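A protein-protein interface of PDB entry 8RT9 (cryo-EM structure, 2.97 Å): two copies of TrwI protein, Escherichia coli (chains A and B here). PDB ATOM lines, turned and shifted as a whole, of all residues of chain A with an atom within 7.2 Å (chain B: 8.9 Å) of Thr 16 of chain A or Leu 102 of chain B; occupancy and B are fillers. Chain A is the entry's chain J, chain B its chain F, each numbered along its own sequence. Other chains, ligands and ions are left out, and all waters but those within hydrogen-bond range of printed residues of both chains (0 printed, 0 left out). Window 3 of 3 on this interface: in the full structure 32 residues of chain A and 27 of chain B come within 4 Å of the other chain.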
ATOM      1  N   PHE A  10      21.536 -21.351   7.456  1.00  0.00           N
ATOM      2  CA  PHE A  10      21.374 -22.730   7.026  1.00  0.00           C
ATOM      3  C   PHE A  10      21.515 -23.683   8.198  1.00  0.00           C
ATOM      4  O   PHE A  10      20.759 -24.652   8.303  1.00  0.00           O
ATOM      5  CB  PHE A  10      22.383 -23.067   5.934  1.00  0.00           C
ATOM      6  CG  PHE A  10      21.959 -22.638   4.564  1.00  0.00           C
ATOM      7  CD1 PHE A  10      21.156 -21.536   4.390  1.00  0.00           C
ATOM      8  CD2 PHE A  10      22.358 -23.342   3.452  1.00  0.00           C
ATOM      9  CE1 PHE A  10      20.770 -21.144   3.137  1.00  0.00           C
ATOM     10  CE2 PHE A  10      21.968 -22.950   2.200  1.00  0.00           C
ATOM     11  CZ  PHE A  10      21.174 -21.851   2.044  1.00  0.00           C
ATOM     12  N   ASN A  11      22.468 -23.426   9.096  1.00  0.00           N
ATOM     13  CA  ASN A  11      22.607 -24.287  10.264  1.00  0.00           C
ATOM     14  C   ASN A  11      21.372 -24.219  11.149  1.00  0.00           C
ATOM     15  O   ASN A  11      20.929 -25.239  11.683  1.00  0.00           O
ATOM     16  CB  ASN A  11      23.854 -23.911  11.054  1.00  0.00           C
ATOM     17  CG  ASN A  11      25.127 -24.291  10.337  1.00  0.00           C
ATOM     18  OD1 ASN A  11      26.004 -23.459  10.122  1.00  0.00           O
ATOM     19  ND2 ASN A  11      25.232 -25.556   9.956  1.00  0.00           N
ATOM     20  N   LYS A  12      20.803 -23.027  11.320  1.00  0.00           N
ATOM     21  CA  LYS A  12      19.603 -22.885  12.136  1.00  0.00           C
ATOM     22  C   LYS A  12      18.438 -23.649  11.531  1.00  0.00           C
ATOM     23  O   LYS A  12      17.723 -24.372  12.234  1.00  0.00           O
ATOM     24  CB  LYS A  12      19.253 -21.408  12.284  1.00  0.00           C
ATOM     25  CG  LYS A  12      17.941 -21.135  12.975  1.00  0.00           C
ATOM     26  CD  LYS A  12      18.127 -21.045  14.470  1.00  0.00           C
ATOM     27  CE  LYS A  12      16.829 -20.701  15.162  1.00  0.00           C
ATOM     28  NZ  LYS A  12      15.784 -21.730  14.917  1.00  0.00           N
ATOM     29  N   ILE A  13      18.232 -23.505  10.223  1.00  0.00           N
ATOM     30  CA  ILE A  13      17.116 -24.189   9.579  1.00  0.00           C
ATOM     31  C   ILE A  13      17.329 -25.695   9.608  1.00  0.00           C
ATOM     32  O   ILE A  13      16.383 -26.468   9.798  1.00  0.00           O
ATOM     33  CB  ILE A  13      16.917 -23.665   8.148  1.00  0.00           C
ATOM     34  CG1 ILE A  13      16.599 -22.175   8.172  1.00  0.00           C
ATOM     35  CG2 ILE A  13      15.804 -24.412   7.460  1.00  0.00           C
ATOM     36  CD1 ILE A  13      15.336 -21.842   8.906  1.00  0.00           C
ATOM     37  N   ASP A  14      18.574 -26.139   9.435  1.00  0.00           N
ATOM     38  CA  ASP A  14      18.860 -27.565   9.489  1.00  0.00           C
ATOM     39  C   ASP A  14      18.638 -28.124  10.886  1.00  0.00           C
ATOM     40  O   ASP A  14      18.109 -29.226  11.037  1.00  0.00           O
ATOM     41  CB  ASP A  14      20.289 -27.831   9.025  1.00  0.00           C
ATOM     42  CG  ASP A  14      20.474 -27.573   7.544  1.00  0.00           C
ATOM     43  OD1 ASP A  14      19.454 -27.431   6.836  1.00  0.00           O
ATOM     44  OD2 ASP A  14      21.634 -27.510   7.087  1.00  0.00           O
ATOM     45  N   GLN A  15      19.036 -27.387  11.919  1.00  0.00           N
ATOM     46  CA  GLN A  15      18.760 -27.841  13.275  1.00  0.00           C
ATOM     47  C   GLN A  15      17.264 -27.910  13.534  1.00  0.00           C
ATOM     48  O   GLN A  15      16.774 -28.873  14.131  1.00  0.00           O
ATOM     49  CB  GLN A  15      19.434 -26.925  14.290  1.00  0.00           C
ATOM     50  CG  GLN A  15      20.761 -27.443  14.787  1.00  0.00           C
ATOM     51  CD  GLN A  15      21.171 -26.811  16.098  1.00  0.00           C
ATOM     52  OE1 GLN A  15      20.685 -25.742  16.461  1.00  0.00           O
ATOM     53  NE2 GLN A  15      22.067 -27.473  16.820  1.00  0.00           N
ATOM     54  N   THR A  16      16.519 -26.901  13.081  1.00  0.00           N
ATOM     55  CA  THR A  16      15.074 -26.915  13.264  1.00  0.00           C
ATOM     56  C   THR A  16      14.444 -28.121  12.589  1.00  0.00           C
ATOM     57  O   THR A  16      13.649 -28.846  13.203  1.00  0.00           O
ATOM     58  CB  THR A  16      14.468 -25.631  12.712  1.00  0.00           C
ATOM     59  OG1 THR A  16      15.013 -24.509  13.412  1.00  0.00           O
ATOM     60  CG2 THR A  16      12.971 -25.642  12.886  1.00  0.00           C
ATOM     61  N   THR A  17      14.795 -28.361  11.327  1.00  0.00           N
ATOM     62  CA  THR A  17      14.195 -29.474  10.608  1.00  0.00           C
ATOM     63  C   THR A  17      14.631 -30.806  11.201  1.00  0.00           C
ATOM     64  O   THR A  17      13.817 -31.724  11.314  1.00  0.00           O
ATOM     65  CB  THR A  17      14.513 -29.382   9.115  1.00  0.00           C
ATOM     66  OG1 THR A  17      13.705 -30.320   8.401  1.00  0.00           O
ATOM     67  CG2 THR A  17      15.964 -29.674   8.831  1.00  0.00           C
ATOM     68  N   ALA A  18      15.878 -30.911  11.655  1.00  0.00           N
ATOM     69  CA  ALA A  18      16.330 -32.142  12.285  1.00  0.00           C
ATOM     70  C   ALA A  18      15.544 -32.427  13.553  1.00  0.00           C
ATOM     71  O   ALA A  18      15.118 -33.562  13.786  1.00  0.00           O
ATOM     72  CB  ALA A  18      17.822 -32.055  12.589  1.00  0.00           C
ATOM     73  N   THR A  19      15.331 -31.409  14.384  1.00  0.00           N
ATOM     74  CA  THR A  19      14.637 -31.634  15.646  1.00  0.00           C
ATOM     75  C   THR A  19      13.159 -31.930  15.439  1.00  0.00           C
ATOM     76  O   THR A  19      12.572 -32.710  16.193  1.00  0.00           O
ATOM     77  CB  THR A  19      14.808 -30.435  16.571  1.00  0.00           C
ATOM     78  OG1 THR A  19      14.239 -29.273  15.958  1.00  0.00           O
ATOM     79  CG2 THR A  19      16.273 -30.200  16.878  1.00  0.00           C
ATOM     80  N   TYR A  20      12.532 -31.322  14.434  1.00  0.00           N
ATOM     81  CA  TYR A  20      11.077 -31.378  14.349  1.00  0.00           C
ATOM     82  C   TYR A  20      10.547 -32.378  13.325  1.00  0.00           C
ATOM     83  O   TYR A  20       9.493 -32.977  13.550  1.00  0.00           O
ATOM     84  CB  TYR A  20      10.531 -29.974  14.086  1.00  0.00           C
ATOM     85  CG  TYR A  20      10.637 -29.115  15.316  1.00  0.00           C
ATOM     86  CD1 TYR A  20      10.066 -29.519  16.508  1.00  0.00           C
ATOM     87  CD2 TYR A  20      11.335 -27.927  15.301  1.00  0.00           C
ATOM     88  CE1 TYR A  20      10.168 -28.758  17.638  1.00  0.00           C
ATOM     89  CE2 TYR A  20      11.441 -27.158  16.431  1.00  0.00           C
ATOM     90  CZ  TYR A  20      10.858 -27.578  17.596  1.00  0.00           C
ATOM     91  OH  TYR A  20      10.959 -26.810  18.730  1.00  0.00           O
ATOM     92  N   VAL A  21      11.230 -32.570  12.198  1.00  0.00           N
ATOM     93  CA  VAL A  21      10.763 -33.547  11.223  1.00  0.00           C
ATOM     94  C   VAL A  21      11.538 -34.851  11.360  1.00  0.00           C
ATOM     95  O   VAL A  21      10.964 -35.915  11.630  1.00  0.00           O
ATOM     96  CB  VAL A  21      10.879 -32.973   9.802  1.00  0.00           C
ATOM     97  CG1 VAL A  21      10.271 -33.926   8.798  1.00  0.00           C
ATOM     98  CG2 VAL A  21      10.216 -31.620   9.730  1.00  0.00           C
ATOM     99  N   THR A  22      12.856 -34.778  11.190  1.00  0.00           N
ATOM    100  CA  THR A  22      13.679 -35.978  11.104  1.00  0.00           C
ATOM    101  C   THR A  22      13.670 -36.764  12.406  1.00  0.00           C
ATOM    102  O   THR A  22      13.469 -37.984  12.402  1.00  0.00           O
ATOM    103  CB  THR A  22      15.105 -35.591  10.725  1.00  0.00           C
ATOM    104  OG1 THR A  22      15.077 -34.745   9.570  1.00  0.00           O
ATOM    105  CG2 THR A  22      15.929 -36.814  10.429  1.00  0.00           C
ATOM    106  N   ASP B  96      -1.439 -20.836  18.987  1.00  0.00           N
ATOM    107  CA  ASP B  96      -0.875 -22.017  19.628  1.00  0.00           C
ATOM    108  C   ASP B  96       0.230 -22.612  18.780  1.00  0.00           C
ATOM    109  O   ASP B  96       1.289 -22.986  19.295  1.00  0.00           O
ATOM    110  CB  ASP B  96      -1.968 -23.049  19.883  1.00  0.00           C
ATOM    111  CG  ASP B  96      -2.953 -22.603  20.942  1.00  0.00           C
ATOM    112  OD1 ASP B  96      -2.553 -21.835  21.842  1.00  0.00           O
ATOM    113  OD2 ASP B  96      -4.128 -23.017  20.871  1.00  0.00           O
ATOM    114  N   GLU B  97       0.006 -22.695  17.474  1.00  0.00           N
ATOM    115  CA  GLU B  97       1.019 -23.232  16.578  1.00  0.00           C
ATOM    116  C   GLU B  97       2.145 -22.234  16.344  1.00  0.00           C
ATOM    117  O   GLU B  97       3.321 -22.607  16.362  1.00  0.00           O
ATOM    118  CB  GLU B  97       0.358 -23.683  15.274  1.00  0.00           C
ATOM    119  CG  GLU B  97      -0.257 -22.577  14.454  1.00  0.00           C
ATOM    120  CD  GLU B  97      -0.965 -23.088  13.212  1.00  0.00           C
ATOM    121  OE1 GLU B  97      -0.991 -24.318  13.005  1.00  0.00           O
ATOM    122  OE2 GLU B  97      -1.536 -22.266  12.466  1.00  0.00           O
ATOM    123  N   LEU B  98       1.824 -20.951  16.146  1.00  0.00           N
ATOM    124  CA  LEU B  98       2.909 -20.024  15.832  1.00  0.00           C
ATOM    125  C   LEU B  98       3.838 -19.812  17.023  1.00  0.00           C
ATOM    126  O   LEU B  98       5.007 -19.458  16.839  1.00  0.00           O
ATOM    127  CB  LEU B  98       2.348 -18.691  15.328  1.00  0.00           C
ATOM    128  CG  LEU B  98       3.376 -17.703  14.757  1.00  0.00           C
ATOM    129  CD1 LEU B  98       2.825 -16.985  13.536  1.00  0.00           C
ATOM    130  CD2 LEU B  98       3.820 -16.683  15.796  1.00  0.00           C
ATOM    131  N   ALA B  99       3.355 -20.043  18.244  1.00  0.00           N
ATOM    132  CA  ALA B  99       4.146 -19.709  19.424  1.00  0.00           C
ATOM    133  C   ALA B  99       5.330 -20.654  19.601  1.00  0.00           C
ATOM    134  O   ALA B  99       6.453 -20.212  19.864  1.00  0.00           O
ATOM    135  CB  ALA B  99       3.258 -19.718  20.669  1.00  0.00           C
ATOM    136  N   SER B 100       5.098 -21.964  19.494  1.00  0.00           N
ATOM    137  CA  SER B 100       6.171 -22.893  19.831  1.00  0.00           C
ATOM    138  C   SER B 100       6.261 -24.133  18.946  1.00  0.00           C
ATOM    139  O   SER B 100       7.048 -25.030  19.272  1.00  0.00           O
ATOM    140  CB  SER B 100       6.034 -23.329  21.296  1.00  0.00           C
ATOM    141  OG  SER B 100       7.047 -24.256  21.647  1.00  0.00           O
ATOM    142  N   ALA B 101       5.493 -24.239  17.857  1.00  0.00           N
ATOM    143  CA  ALA B 101       5.528 -25.460  17.055  1.00  0.00           C
ATOM    144  C   ALA B 101       6.904 -25.679  16.441  1.00  0.00           C
ATOM    145  O   ALA B 101       7.439 -26.794  16.467  1.00  0.00           O
ATOM    146  CB  ALA B 101       4.455 -25.415  15.967  1.00  0.00           C
ATOM    147  N   LEU B 102       7.496 -24.625  15.881  1.00  0.00           N
ATOM    148  CA  LEU B 102       8.826 -24.706  15.298  1.00  0.00           C
ATOM    149  C   LEU B 102       9.804 -23.692  15.869  1.00  0.00           C
ATOM    150  O   LEU B 102      10.995 -23.762  15.543  1.00  0.00           O
ATOM    151  CB  LEU B 102       8.760 -24.530  13.772  1.00  0.00           C
ATOM    152  CG  LEU B 102       8.440 -25.769  12.933  1.00  0.00           C
ATOM    153  CD1 LEU B 102       6.964 -26.125  13.003  1.00  0.00           C
ATOM    154  CD2 LEU B 102       8.874 -25.559  11.493  1.00  0.00           C
ATOM    155  N   LEU B 103       9.344 -22.751  16.698  1.00  0.00           N
ATOM    156  CA  LEU B 103      10.256 -21.784  17.298  1.00  0.00           C
ATOM    157  C   LEU B 103      11.203 -22.454  18.285  1.00  0.00           C
ATOM    158  O   LEU B 103      12.409 -22.184  18.287  1.00  0.00           O
ATOM    159  CB  LEU B 103       9.466 -20.673  17.991  1.00  0.00           C
ATOM    160  CG  LEU B 103       8.679 -19.739  17.078  1.00  0.00           C
ATOM    161  CD1 LEU B 103       8.132 -18.573  17.861  1.00  0.00           C
ATOM    162  CD2 LEU B 103       9.582 -19.243  15.981  1.00  0.00           C
ATOM    163  N   GLY B 104      10.675 -23.333  19.130  1.00  0.00           N
ATOM    164  CA  GLY B 104      11.464 -23.899  20.201  1.00  0.00           C
ATOM    165  C   GLY B 104      11.651 -22.992  21.394  1.00  0.00           C
ATOM    166  O   GLY B 104      12.463 -23.308  22.271  1.00  0.00           O
ATOM    167  N   ASN B 105      10.930 -21.873  21.456  1.00  0.00           N
ATOM    168  CA  ASN B 105      11.017 -20.928  22.556  1.00  0.00           C
ATOM    169  C   ASN B 105       9.656 -20.792  23.224  1.00  0.00           C
ATOM    170  O   ASN B 105       8.712 -20.289  22.599  1.00  0.00           O
ATOM    171  CB  ASN B 105      11.497 -19.554  22.061  1.00  0.00           C
ATOM    172  N   VAL B 211      -1.819 -23.250   8.743  1.00  0.00           N
ATOM    173  CA  VAL B 211      -0.776 -23.989   9.451  1.00  0.00           C
ATOM    174  C   VAL B 211       0.599 -23.612   8.915  1.00  0.00           C
ATOM    175  O   VAL B 211       1.517 -23.280   9.679  1.00  0.00           O
ATOM    176  CB  VAL B 211      -1.024 -25.501   9.348  1.00  0.00           C
ATOM    177  CG1 VAL B 211       0.151 -26.264   9.909  1.00  0.00           C
ATOM    178  CG2 VAL B 211      -2.283 -25.875  10.089  1.00  0.00           C
ATOM    179  N   LEU B 212       0.758 -23.645   7.590  1.00  0.00           N
ATOM    180  CA  LEU B 212       2.055 -23.364   6.986  1.00  0.00           C
ATOM    181  C   LEU B 212       2.519 -21.948   7.296  1.00  0.00           C
ATOM    182  O   LEU B 212       3.668 -21.738   7.704  1.00  0.00           O
ATOM    183  CB  LEU B 212       1.985 -23.586   5.477  1.00  0.00           C
ATOM    184  CG  LEU B 212       1.844 -25.021   4.975  1.00  0.00           C
ATOM    185  CD1 LEU B 212       1.272 -25.030   3.576  1.00  0.00           C
ATOM    186  CD2 LEU B 212       3.177 -25.724   5.000  1.00  0.00           C
ATOM    187  N   ALA B 214       1.497 -19.882   9.793  1.00  0.00           N
ATOM    188  CA  ALA B 214       1.820 -19.694  11.198  1.00  0.00           C
ATOM    189  C   ALA B 214       3.196 -20.261  11.519  1.00  0.00           C
ATOM    190  O   ALA B 214       4.069 -19.545  12.016  1.00  0.00           O
ATOM    191  CB  ALA B 214       0.748 -20.323  12.072  1.00  0.00           C
ATOM    192  N   ALA B 215       3.440 -21.521  11.156  1.00  0.00           N
ATOM    193  CA  ALA B 215       4.706 -22.156  11.508  1.00  0.00           C
ATOM    194  C   ALA B 215       5.892 -21.439  10.869  1.00  0.00           C
ATOM    195  O   ALA B 215       6.775 -20.911  11.566  1.00  0.00           O
ATOM    196  CB  ALA B 215       4.676 -23.625  11.094  1.00  0.00           C
ATOM    197  N   VAL B 216       5.934 -21.417   9.537  1.00  0.00           N
ATOM    198  CA  VAL B 216       7.109 -20.905   8.844  1.00  0.00           C
ATOM    199  C   VAL B 216       7.282 -19.414   9.096  1.00  0.00           C
ATOM    200  O   VAL B 216       8.404 -18.936   9.293  1.00  0.00           O
ATOM    201  CB  VAL B 216       7.015 -21.218   7.342  1.00  0.00           C
ATOM    202  CG1 VAL B 216       8.180 -20.608   6.600  1.00  0.00           C
ATOM    203  CG2 VAL B 216       6.980 -22.714   7.126  1.00  0.00           C
ATOM    204  N   PHE B 217       6.192 -18.650   9.059  1.00  0.00           N
ATOM    205  CA  PHE B 217       6.269 -17.222   9.305  1.00  0.00           C
ATOM    206  C   PHE B 217       6.750 -16.923  10.712  1.00  0.00           C
ATOM    207  O   PHE B 217       7.548 -16.006  10.907  1.00  0.00           O
ATOM    208  CB  PHE B 217       4.909 -16.579   9.066  1.00  0.00           C
ATOM    209  CG  PHE B 217       4.932 -15.088   9.119  1.00  0.00           C
ATOM    210  CD1 PHE B 217       5.898 -14.376   8.446  1.00  0.00           C
ATOM    211  CD2 PHE B 217       3.991 -14.399   9.846  1.00  0.00           C
ATOM    212  CE1 PHE B 217       5.922 -13.006   8.494  1.00  0.00           C
ATOM    213  CE2 PHE B 217       4.011 -13.030   9.897  1.00  0.00           C
ATOM    214  CZ  PHE B 217       4.981 -12.333   9.225  1.00  0.00           C
ATOM    215  N   GLY B 218       6.279 -17.666  11.711  1.00  0.00           N
ATOM    216  CA  GLY B 218       6.794 -17.458  13.048  1.00  0.00           C
ATOM    217  C   GLY B 218       8.286 -17.695  13.118  1.00  0.00           C
ATOM    218  O   GLY B 218       9.031 -16.885  13.674  1.00  0.00           O
ATOM    219  N   LEU B 219       8.747 -18.796  12.523  1.00  0.00           N
ATOM    220  CA  LEU B 219      10.178 -19.085  12.544  1.00  0.00           C
ATOM    221  C   LEU B 219      10.975 -17.975  11.871  1.00  0.00           C
ATOM    222  O   LEU B 219      11.941 -17.447  12.439  1.00  0.00           O
ATOM    223  CB  LEU B 219      10.447 -20.426  11.871  1.00  0.00           C
ATOM    224  CG  LEU B 219      11.894 -20.897  11.882  1.00  0.00           C
ATOM    225  CD1 LEU B 219      12.354 -21.134  13.301  1.00  0.00           C
ATOM    226  CD2 LEU B 219      12.040 -22.155  11.061  1.00  0.00           C
ATOM    227  N   LEU B 220      10.562 -17.588  10.665  1.00  0.00           N
ATOM    228  CA  LEU B 220      11.313 -16.603   9.896  1.00  0.00           C
ATOM    229  C   LEU B 220      11.282 -15.237  10.559  1.00  0.00           C
ATOM    230  O   LEU B 220      12.299 -14.535  10.599  1.00  0.00           O
ATOM    231  CB  LEU B 220      10.756 -16.522   8.480  1.00  0.00           C
ATOM    232  CG  LEU B 220      11.017 -17.751   7.616  1.00  0.00           C
ATOM    233  CD1 LEU B 220      10.427 -17.568   6.237  1.00  0.00           C
ATOM    234  CD2 LEU B 220      12.497 -18.022   7.530  1.00  0.00           C
ATOM    235  N   GLN B 222      10.829 -14.567  13.754  1.00  0.00           N
ATOM    236  CA  GLN B 222      11.657 -14.595  14.950  1.00  0.00           C
ATOM    237  C   GLN B 222      13.136 -14.492  14.600  1.00  0.00           C
ATOM    238  O   GLN B 222      13.893 -13.782  15.276  1.00  0.00           O
ATOM    239  CB  GLN B 222      11.369 -15.865  15.744  1.00  0.00           C
ATOM    240  CG  GLN B 222      12.025 -15.922  17.101  1.00  0.00           C
ATOM    241  CD  GLN B 222      13.390 -16.570  17.058  1.00  0.00           C
ATOM    242  OE1 GLN B 222      13.624 -17.496  16.283  1.00  0.00           O
ATOM    243  NE2 GLN B 222      14.303 -16.085  17.891  1.00  0.00           N
ATOM    244  N   ILE B 223      13.568 -15.186  13.545  1.00  0.00           N
ATOM    245  CA  ILE B 223      14.963 -15.088  13.121  1.00  0.00           C
ATOM    246  C   ILE B 223      15.298 -13.653  12.737  1.00  0.00           C
ATOM    247  O   ILE B 223      16.322 -13.094  13.158  1.00  0.00           O
ATOM    248  CB  ILE B 223      15.241 -16.057  11.960  1.00  0.00           C
ATOM    249  CG1 ILE B 223      15.300 -17.494  12.465  1.00  0.00           C
ATOM    250  CG2 ILE B 223      16.531 -15.696  11.263  1.00  0.00           C
ATOM    251  CD1 ILE B 223      15.244 -18.517  11.370  1.00  0.00           C
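Among the printed residues, pairs that only touch across the chains: Lys 12 of chain A with Leu 219 of chain B (3.8 Å), Ile 13 of chain A with Leu 219 of chain B (3.95 Å), Thr 16 of chain A with Leu 102 of chain B (3.8 Å), Tyr 20 of chain A with Ala 101 of chain B (3.6 Å), Tyr 20 of chain A with Leu 102 of chain B (3.5 Å) and Tyr 20 of chain A with Gly 104 of chain B (3.3 Å).
Along chain B the printed residues that touch a printed residue of chain A span positions 101 to 219. Printed residues of chain A that touch a printed residue of chain B: Lys 12, Ile 13, Thr 16 and Tyr 20. Among the printed residues, no Asp or Glu carboxylate lies within 4 Å of a Lys or Arg side-chain nitrogen of the other chain.
The backbone carbonyl oxygen (O) of Lys 12 of chain A sits at hydrogen-bond distance from the side-chain hydroxyl (OG1) of Thr 16 of chain A (3.0 Å). OG1 of Thr 19 of chain A sits at hydrogen-bond distance from O of Thr 16 of chain A, 2.8 Å away.
Of chain B, only Leu 102 comes within 4 Å of Thr 16 of chain A. No residue of chain B comes within 4 Å of Thr 17 of chain A. Ala 101 of chain B touches just one residue of chain A: Tyr 20. Of the printed residues of chain B, Tyr 20 of chain A touches Ala 101, Leu 102 and Gly 104. Of the printed residues of chain A, Gly 104 of chain B touches Tyr 20 (3.3 Å). Val 21 of chain A touches none of the printed residues of chain B. The nearest residue of chain A that does not touch Leu 102 of chain B is Lys 12 of chain A (5.2 Å). The nearest printed residue of chain B that does not touch Tyr 20 of chain A is Ser 100 of chain B (4.3 Å).
No position is printed for both chains.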
